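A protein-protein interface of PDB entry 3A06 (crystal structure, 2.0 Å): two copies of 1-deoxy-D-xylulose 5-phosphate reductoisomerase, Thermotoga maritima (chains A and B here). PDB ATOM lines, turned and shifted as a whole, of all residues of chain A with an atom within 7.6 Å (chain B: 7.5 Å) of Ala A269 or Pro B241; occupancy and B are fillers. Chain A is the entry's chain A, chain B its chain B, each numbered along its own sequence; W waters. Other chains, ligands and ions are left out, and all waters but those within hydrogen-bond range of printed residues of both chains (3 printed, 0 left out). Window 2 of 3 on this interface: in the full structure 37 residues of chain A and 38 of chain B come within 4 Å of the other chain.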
ATOM      1  N   LYS A  25      17.405  12.598 -40.080  1.00  0.00           N
ATOM      2  CA  LYS A  25      17.603  11.534 -39.090  1.00  0.00           C
ATOM      3  C   LYS A  25      16.473  11.449 -38.075  1.00  0.00           C
ATOM      4  O   LYS A  25      16.325  10.451 -37.359  1.00  0.00           O
ATOM      5  CB  LYS A  25      18.932  11.717 -38.356  1.00  0.00           C
ATOM      6  CG  LYS A  25      20.161  11.576 -39.223  1.00  0.00           C
ATOM      7  CD  LYS A  25      21.382  12.227 -38.564  1.00  0.00           C
ATOM      8  CE  LYS A  25      22.188  11.235 -37.727  1.00  0.00           C
ATOM      9  NZ  LYS A  25      23.071  10.378 -38.592  1.00  0.00           N
ATOM     10  N   VAL A  26      15.667  12.498 -37.997  1.00  0.00           N
ATOM     11  CA  VAL A  26      14.644  12.549 -36.981  1.00  0.00           C
ATOM     12  C   VAL A  26      13.427  13.261 -37.547  1.00  0.00           C
ATOM     13  O   VAL A  26      13.564  14.200 -38.320  1.00  0.00           O
ATOM     14  CB  VAL A  26      15.185  13.145 -35.633  1.00  0.00           C
ATOM     15  CG1 VAL A  26      16.035  14.344 -35.855  1.00  0.00           C
ATOM     16  CG2 VAL A  26      14.074  13.466 -34.668  1.00  0.00           C
ATOM     17  N   SER A 259      20.360  19.057 -32.600  1.00  0.00           N
ATOM     18  CA  SER A 259      19.180  18.215 -32.396  1.00  0.00           C
ATOM     19  C   SER A 259      18.506  18.592 -31.086  1.00  0.00           C
ATOM     20  O   SER A 259      17.276  18.649 -31.011  1.00  0.00           O
ATOM     21  CB  SER A 259      19.533  16.729 -32.452  1.00  0.00           C
ATOM     22  OG  SER A 259      20.199  16.306 -31.242  1.00  0.00           O
ATOM     23  N   ARG A 266      12.264  17.094 -25.916  1.00  0.00           N
ATOM     24  CA  ARG A 266      12.527  15.702 -26.268  1.00  0.00           C
ATOM     25  C   ARG A 266      14.024  15.494 -26.531  1.00  0.00           C
ATOM     26  O   ARG A 266      14.718  16.417 -26.965  1.00  0.00           O
ATOM     27  CB  ARG A 266      11.731  15.291 -27.508  1.00  0.00           C
ATOM     28  CG  ARG A 266      10.192  15.338 -27.336  1.00  0.00           C
ATOM     29  CD  ARG A 266       9.668  14.173 -26.488  1.00  0.00           C
ATOM     30  NE  ARG A 266       8.626  13.425 -27.199  1.00  0.00           N
ATOM     31  CZ  ARG A 266       8.753  12.165 -27.614  1.00  0.00           C
ATOM     32  NH1 ARG A 266       9.878  11.472 -27.380  1.00  0.00           N
ATOM     33  NH2 ARG A 266       7.750  11.590 -28.262  1.00  0.00           N
ATOM     34  N   ARG A 267      14.507  14.294 -26.248  1.00  0.00           N
ATOM     35  CA  ARG A 267      15.868  13.888 -26.588  1.00  0.00           C
ATOM     36  C   ARG A 267      15.749  13.058 -27.840  1.00  0.00           C
ATOM     37  O   ARG A 267      14.953  12.106 -27.875  1.00  0.00           O
ATOM     38  CB  ARG A 267      16.453  13.020 -25.455  1.00  0.00           C
ATOM     39  CG  ARG A 267      16.714  13.746 -24.155  1.00  0.00           C
ATOM     40  CD  ARG A 267      18.054  14.521 -24.256  1.00  0.00           C
ATOM     41  NE  ARG A 267      18.384  15.260 -23.039  1.00  0.00           N
ATOM     42  CZ  ARG A 267      19.484  15.985 -22.893  1.00  0.00           C
ATOM     43  NH1 ARG A 267      20.351  16.078 -23.894  1.00  0.00           N
ATOM     44  NH2 ARG A 267      19.730  16.609 -21.739  1.00  0.00           N
ATOM     45  N   VAL A 268      16.539  13.387 -28.852  1.00  0.00           N
ATOM     46  CA  VAL A 268      16.559  12.659 -30.115  1.00  0.00           C
ATOM     47  C   VAL A 268      17.433  11.403 -30.017  1.00  0.00           C
ATOM     48  O   VAL A 268      18.475  11.425 -29.356  1.00  0.00           O
ATOM     49  CB  VAL A 268      17.112  13.572 -31.227  1.00  0.00           C
ATOM     50  CG1 VAL A 268      17.295  12.815 -32.512  1.00  0.00           C
ATOM     51  CG2 VAL A 268      16.144  14.701 -31.466  1.00  0.00           C
ATOM     52  N   ALA A 269      17.010  10.323 -30.678  1.00  0.00           N
ATOM     53  CA  ALA A 269      17.819   9.104 -30.739  1.00  0.00           C
ATOM     54  C   ALA A 269      18.874   9.216 -31.823  1.00  0.00           C
ATOM     55  O   ALA A 269      18.565   9.123 -33.001  1.00  0.00           O
ATOM     56  CB  ALA A 269      16.924   7.880 -30.981  1.00  0.00           C
ATOM     57  N   LEU A 270      20.124   9.463 -31.432  1.00  0.00           N
ATOM     58  CA  LEU A 270      21.208   9.485 -32.392  1.00  0.00           C
ATOM     59  C   LEU A 270      22.069   8.291 -32.040  1.00  0.00           C
ATOM     60  O   LEU A 270      21.635   7.168 -32.243  1.00  0.00           O
ATOM     61  CB  LEU A 270      21.995  10.793 -32.346  1.00  0.00           C
ATOM     62  CG  LEU A 270      21.179  12.028 -32.731  1.00  0.00           C
ATOM     63  CD1 LEU A 270      21.977  13.287 -32.467  1.00  0.00           C
ATOM     64  CD2 LEU A 270      20.697  11.959 -34.210  1.00  0.00           C
ATOM     65  N   GLU A 271      23.249   8.516 -31.482  1.00  0.00           N
ATOM     66  CA  GLU A 271      24.044   7.383 -31.000  1.00  0.00           C
ATOM     67  C   GLU A 271      24.570   7.659 -29.601  1.00  0.00           C
ATOM     68  O   GLU A 271      25.309   8.618 -29.391  1.00  0.00           O
ATOM     69  CB  GLU A 271      25.169   7.028 -31.980  1.00  0.00           C
ATOM     70  CG  GLU A 271      25.275   5.503 -32.271  1.00  0.00           C
ATOM     71  CD  GLU A 271      24.021   4.896 -32.945  1.00  0.00           C
ATOM     72  OE1 GLU A 271      23.543   3.848 -32.447  1.00  0.00           O
ATOM     73  OE2 GLU A 271      23.514   5.460 -33.956  1.00  0.00           O
ATOM     74  N   PRO A 272      24.154   6.831 -28.634  1.00  0.00           N
ATOM     75  CA  PRO A 272      24.552   7.007 -27.236  1.00  0.00           C
ATOM     76  C   PRO A 272      26.063   6.866 -27.071  1.00  0.00           C
ATOM     77  O   PRO A 272      26.698   6.112 -27.818  1.00  0.00           O
ATOM     78  CB  PRO A 272      23.797   5.891 -26.510  1.00  0.00           C
ATOM     79  CG  PRO A 272      22.654   5.553 -27.443  1.00  0.00           C
ATOM     80  CD  PRO A 272      23.241   5.690 -28.807  1.00  0.00           C
ATOM     81  N   PHE A 273      26.622   7.625 -26.130  1.00  0.00           N
ATOM     82  CA  PHE A 273      28.059   7.693 -25.924  1.00  0.00           C
ATOM     83  C   PHE A 273      28.400   6.785 -24.774  1.00  0.00           C
ATOM     84  O   PHE A 273      28.101   7.099 -23.622  1.00  0.00           O
ATOM     85  CB  PHE A 273      28.490   9.118 -25.578  1.00  0.00           C
ATOM     86  CG  PHE A 273      29.985   9.376 -25.733  1.00  0.00           C
ATOM     87  CD1 PHE A 273      30.708   8.824 -26.790  1.00  0.00           C
ATOM     88  CD2 PHE A 273      30.652  10.215 -24.849  1.00  0.00           C
ATOM     89  CE1 PHE A 273      32.080   9.082 -26.947  1.00  0.00           C
ATOM     90  CE2 PHE A 273      32.033  10.469 -24.997  1.00  0.00           C
ATOM     91  CZ  PHE A 273      32.738   9.903 -26.038  1.00  0.00           C
ATOM     92  N   GLU B 153      16.321  12.542 -16.131  1.00  0.00           N
ATOM     93  CA  GLU B 153      15.206  13.030 -16.944  1.00  0.00           C
ATOM     94  C   GLU B 153      14.480  11.828 -17.543  1.00  0.00           C
ATOM     95  O   GLU B 153      15.063  10.753 -17.616  1.00  0.00           O
ATOM     96  CB  GLU B 153      15.699  14.013 -18.026  1.00  0.00           C
ATOM     97  CG  GLU B 153      16.908  13.574 -18.797  1.00  0.00           C
ATOM     98  CD  GLU B 153      17.302  14.613 -19.861  1.00  0.00           C
ATOM     99  OE1 GLU B 153      18.241  15.409 -19.627  1.00  0.00           O
ATOM    100  OE2 GLU B 153      16.641  14.654 -20.921  1.00  0.00           O
ATOM    101  N   GLU B 155      13.670  10.711 -20.548  1.00  0.00           N
ATOM    102  CA  GLU B 155      14.142   9.959 -21.705  1.00  0.00           C
ATOM    103  C   GLU B 155      15.609   9.457 -21.643  1.00  0.00           C
ATOM    104  O   GLU B 155      16.262   9.323 -22.658  1.00  0.00           O
ATOM    105  CB  GLU B 155      13.835  10.726 -23.012  1.00  0.00           C
ATOM    106  CG  GLU B 155      12.358  11.118 -23.164  1.00  0.00           C
ATOM    107  CD  GLU B 155      12.068  12.011 -24.404  1.00  0.00           C
ATOM    108  OE1 GLU B 155      11.157  12.857 -24.320  1.00  0.00           O
ATOM    109  OE2 GLU B 155      12.737  11.884 -25.438  1.00  0.00           O
ATOM    110  N   VAL B 156      16.109   9.105 -20.465  1.00  0.00           N
ATOM    111  CA  VAL B 156      17.461   8.519 -20.375  1.00  0.00           C
ATOM    112  C   VAL B 156      17.560   7.196 -21.124  1.00  0.00           C
ATOM    113  O   VAL B 156      16.582   6.429 -21.203  1.00  0.00           O
ATOM    114  CB  VAL B 156      17.917   8.336 -18.908  1.00  0.00           C
ATOM    115  CG1 VAL B 156      17.887   9.697 -18.185  1.00  0.00           C
ATOM    116  CG2 VAL B 156      17.015   7.357 -18.190  1.00  0.00           C
ATOM    117  N   GLU B 157      18.738   6.933 -21.676  1.00  0.00           N
ATOM    118  CA  GLU B 157      19.062   5.665 -22.297  1.00  0.00           C
ATOM    119  C   GLU B 157      19.615   4.688 -21.236  1.00  0.00           C
ATOM    120  O   GLU B 157      19.226   3.528 -21.193  1.00  0.00           O
ATOM    121  CB  GLU B 157      20.097   5.871 -23.399  1.00  0.00           C
ATOM    122  CG  GLU B 157      20.569   4.597 -24.099  1.00  0.00           C
ATOM    123  CD  GLU B 157      19.917   4.353 -25.467  1.00  0.00           C
ATOM    124  OE1 GLU B 157      19.527   5.343 -26.144  1.00  0.00           O
ATOM    125  OE2 GLU B 157      19.817   3.161 -25.881  1.00  0.00           O
ATOM    126  N   LYS B 158      20.531   5.162 -20.400  1.00  0.00           N
ATOM    127  CA  LYS B 158      21.095   4.329 -19.352  1.00  0.00           C
ATOM    128  C   LYS B 158      21.372   5.201 -18.158  1.00  0.00           C
ATOM    129  O   LYS B 158      21.820   6.349 -18.305  1.00  0.00           O
ATOM    130  CB  LYS B 158      22.390   3.654 -19.836  1.00  0.00           C
ATOM    131  CG  LYS B 158      22.462   2.139 -19.557  1.00  0.00           C
ATOM    132  CD  LYS B 158      21.427   1.363 -20.344  1.00  0.00           C
ATOM    133  CE  LYS B 158      22.014   0.166 -21.078  1.00  0.00           C
ATOM    134  NZ  LYS B 158      21.344  -0.010 -22.410  1.00  0.00           N
ATOM    135  N   VAL B 238      23.987   9.886 -16.317  1.00  0.00           N
ATOM    136  CA  VAL B 238      22.903   9.461 -17.169  1.00  0.00           C
ATOM    137  C   VAL B 238      23.394   9.570 -18.603  1.00  0.00           C
ATOM    138  O   VAL B 238      23.994  10.597 -19.001  1.00  0.00           O
ATOM    139  CB  VAL B 238      21.535  10.223 -16.932  1.00  0.00           C
ATOM    140  CG1 VAL B 238      21.027  10.031 -15.473  1.00  0.00           C
ATOM    141  CG2 VAL B 238      21.678  11.699 -17.239  1.00  0.00           C
ATOM    142  N   VAL B 239      23.141   8.509 -19.358  1.00  0.00           N
ATOM    143  CA  VAL B 239      23.477   8.435 -20.792  1.00  0.00           C
ATOM    144  C   VAL B 239      22.183   8.762 -21.542  1.00  0.00           C
ATOM    145  O   VAL B 239      21.140   8.132 -21.298  1.00  0.00           O
ATOM    146  CB  VAL B 239      24.074   7.050 -21.184  1.00  0.00           C
ATOM    147  CG1 VAL B 239      24.377   6.953 -22.683  1.00  0.00           C
ATOM    148  CG2 VAL B 239      25.356   6.773 -20.378  1.00  0.00           C
ATOM    149  N   LEU B 240      22.228   9.801 -22.391  1.00  0.00           N
ATOM    150  CA  LEU B 240      21.038  10.220 -23.143  1.00  0.00           C
ATOM    151  C   LEU B 240      21.049   9.632 -24.560  1.00  0.00           C
ATOM    152  O   LEU B 240      22.112   9.308 -25.088  1.00  0.00           O
ATOM    153  CB  LEU B 240      20.955  11.748 -23.183  1.00  0.00           C
ATOM    154  CG  LEU B 240      20.900  12.208 -21.708  1.00  0.00           C
ATOM    155  CD1 LEU B 240      21.479  13.548 -21.455  1.00  0.00           C
ATOM    156  CD2 LEU B 240      19.502  12.039 -21.137  1.00  0.00           C
ATOM    157  N   PRO B 241      19.875   9.516 -25.187  1.00  0.00           N
ATOM    158  CA  PRO B 241      19.862   8.870 -26.505  1.00  0.00           C
ATOM    159  C   PRO B 241      20.551   9.673 -27.625  1.00  0.00           C
ATOM    160  O   PRO B 241      20.781   9.118 -28.714  1.00  0.00           O
ATOM    161  CB  PRO B 241      18.369   8.674 -26.820  1.00  0.00           C
ATOM    162  CG  PRO B 241      17.577   9.324 -25.716  1.00  0.00           C
ATOM    163  CD  PRO B 241      18.540   9.951 -24.721  1.00  0.00           C
ATOM    164  N   ASP B 242      20.867  10.946 -27.357  1.00  0.00           N
ATOM    165  CA  ASP B 242      21.469  11.826 -28.365  1.00  0.00           C
ATOM    166  C   ASP B 242      22.999  11.830 -28.400  1.00  0.00           C
ATOM    167  O   ASP B 242      23.575  12.384 -29.334  1.00  0.00           O
ATOM    168  CB  ASP B 242      20.932  13.287 -28.268  1.00  0.00           C
ATOM    169  CG  ASP B 242      21.142  13.946 -26.872  1.00  0.00           C
ATOM    170  OD1 ASP B 242      21.790  13.327 -25.984  1.00  0.00           O
ATOM    171  OD2 ASP B 242      20.653  15.098 -26.664  1.00  0.00           O
ATOM    172  N   GLY B 243      23.664  11.226 -27.404  1.00  0.00           N
ATOM    173  CA  GLY B 243      25.134  11.255 -27.356  1.00  0.00           C
ATOM    174  C   GLY B 243      25.695  12.018 -26.163  1.00  0.00           C
ATOM    175  O   GLY B 243      26.874  11.913 -25.829  1.00  0.00           O
ATOM    176  N   ASN B 244      24.845  12.800 -25.519  1.00  0.00           N
ATOM    177  CA  ASN B 244      25.227  13.570 -24.349  1.00  0.00           C
ATOM    178  C   ASN B 244      25.286  12.604 -23.144  1.00  0.00           C
ATOM    179  O   ASN B 244      24.529  11.623 -23.068  1.00  0.00           O
ATOM    180  CB  ASN B 244      24.158  14.641 -24.070  1.00  0.00           C
ATOM    181  CG  ASN B 244      24.328  15.925 -24.920  1.00  0.00           C
ATOM    182  OD1 ASN B 244      23.377  16.410 -25.561  1.00  0.00           O
ATOM    183  ND2 ASN B 244      25.521  16.488 -24.898  1.00  0.00           N
HETATM  184  O   HOH W   1      19.475  18.336 -18.750  1.00  0.00           O
HETATM  185  O   HOH W   2      24.836   9.371 -24.844  1.00  0.00           O
HETATM  186  O   HOH W   3      25.014  10.812 -30.982  1.00  0.00           O
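Among the printed residues, merely in contact across the chains: Arg A267 with Leu B240, Arg A267 with Pro B241, Ala A269 with Pro B241, Leu A270 with Asp B242, Glu A271 with Pro B241, Glu A271 with Gly B243, Pro A272 with Glu B157, Pro A272 with Leu B240, Phe A273 with Val B239 and Phe A273 with Gly B243.
Printed residues of chain B that touch a printed residue of chain A: Glu B153, Glu B155, Glu B157, Val B239, Leu B240, Pro B241, Asp B242, Gly B243 and Asn B244.
Hydrophobic or aromatic side chains of chain B within 4 Å of the printed part of chain A: Val B239, Leu B240 and Pro B241.
Hydrophobic or aromatic side chains of chain A within 4 Å of the printed part of chain B: Leu A270, Pro A272 and Phe A273.
Water W3 lies within hydrogen-bond range of the backbone carbonyl oxygen of Asp B242 (2.7 Å) and the backbone carbonyl oxygen of Glu A271 (2.7 Å).
Water W2 lies within hydrogen-bond range of O of Leu B240, N of Phe A273, O of Asn B244 and N of Gly B243.
Water W1 lies within hydrogen-bond range of OE1 of Glu B153 and NH2 of Arg A267.
No position is printed for both chains.
Of the 18 pairs that touch across the chains among the printed residues, none has its exchanged pair printed and touching as well.
Ala A269 touches just one residue of chain B: Pro B241 (3.6 Å).
Of chain A, only Arg A267, Val A268, Ala A269, Leu A270 and Glu A271 come within 4 Å of Pro B241.
Printed residues of chain A within 4 Å of Asn B244: Arg A267 (3.5 Å).
Of the printed residues of chain B, Phe A273 touches Val B239 (3.8 Å) and Gly B243 (3.2 Å).
Of the printed residues of chain B, Arg A267 touches Glu B153, Glu B155, Leu B240, Pro B241, Asp B242 and Asn B244.
Printed residues of chain A within 4 Å of Leu B240: Arg A267 and Pro A272.
Of the printed residues of chain A, Val B239 touches Phe A273.
The nearest residue of chain B that does not touch Ala A269 is Asp B242 (4.9 Å).
The nearest residue of chain A that does not touch Pro B241 is Pro A272 (4.1 Å).
The nearest printed residue of chain A that does not touch Leu B240 is Phe A273 (4.9 Å).
O of Val B239 sits at hydrogen-bond distance from N of Glu B157, at 2.7 Å.
The backbone NH of Val B239 sits at hydrogen-bond distance from the backbone carbonyl oxygen of Lys B158, at 2.7 Å.
The backbone NH (N) of Asn B244 is in hydrogen-bond range of the side-chain carboxylate (OD1) of Asp B242 (3.1 Å).
The side-chain carboxylate (OE2) of Glu B155 is in salt-bridge range of the guanidinium group (NH1) of Arg A266 (3.5 Å).
The side-chain carboxylate of Glu B153 lies within salt-bridge range of the guanidinium group of Arg A267.
The backbone NH (N) of Arg A267 sits at hydrogen-bond distance from the side-chain carboxylate (OE2) of Glu B155 (3.1 Å).
The guanidinium group of Arg A267 lies within salt-bridge range of the side-chain carboxylate of Asp B242, at 3.0 Å.
The guanidinium group of Arg A267 sits at hydrogen-bond distance from the side-chain amide oxygen of Asn B244 (3.5 Å).
The backbone carbonyl oxygen (O) of Val A268 sits at hydrogen-bond distance from the backbone NH (N) of Asp B242 (3.2 Å).
N of Leu A270 is in hydrogen-bond range of O of Pro B241.
The backbone carbonyl oxygen of Val A268 lies close to the backbone carbonyl oxygen of Pro B241 (3.3 Å).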
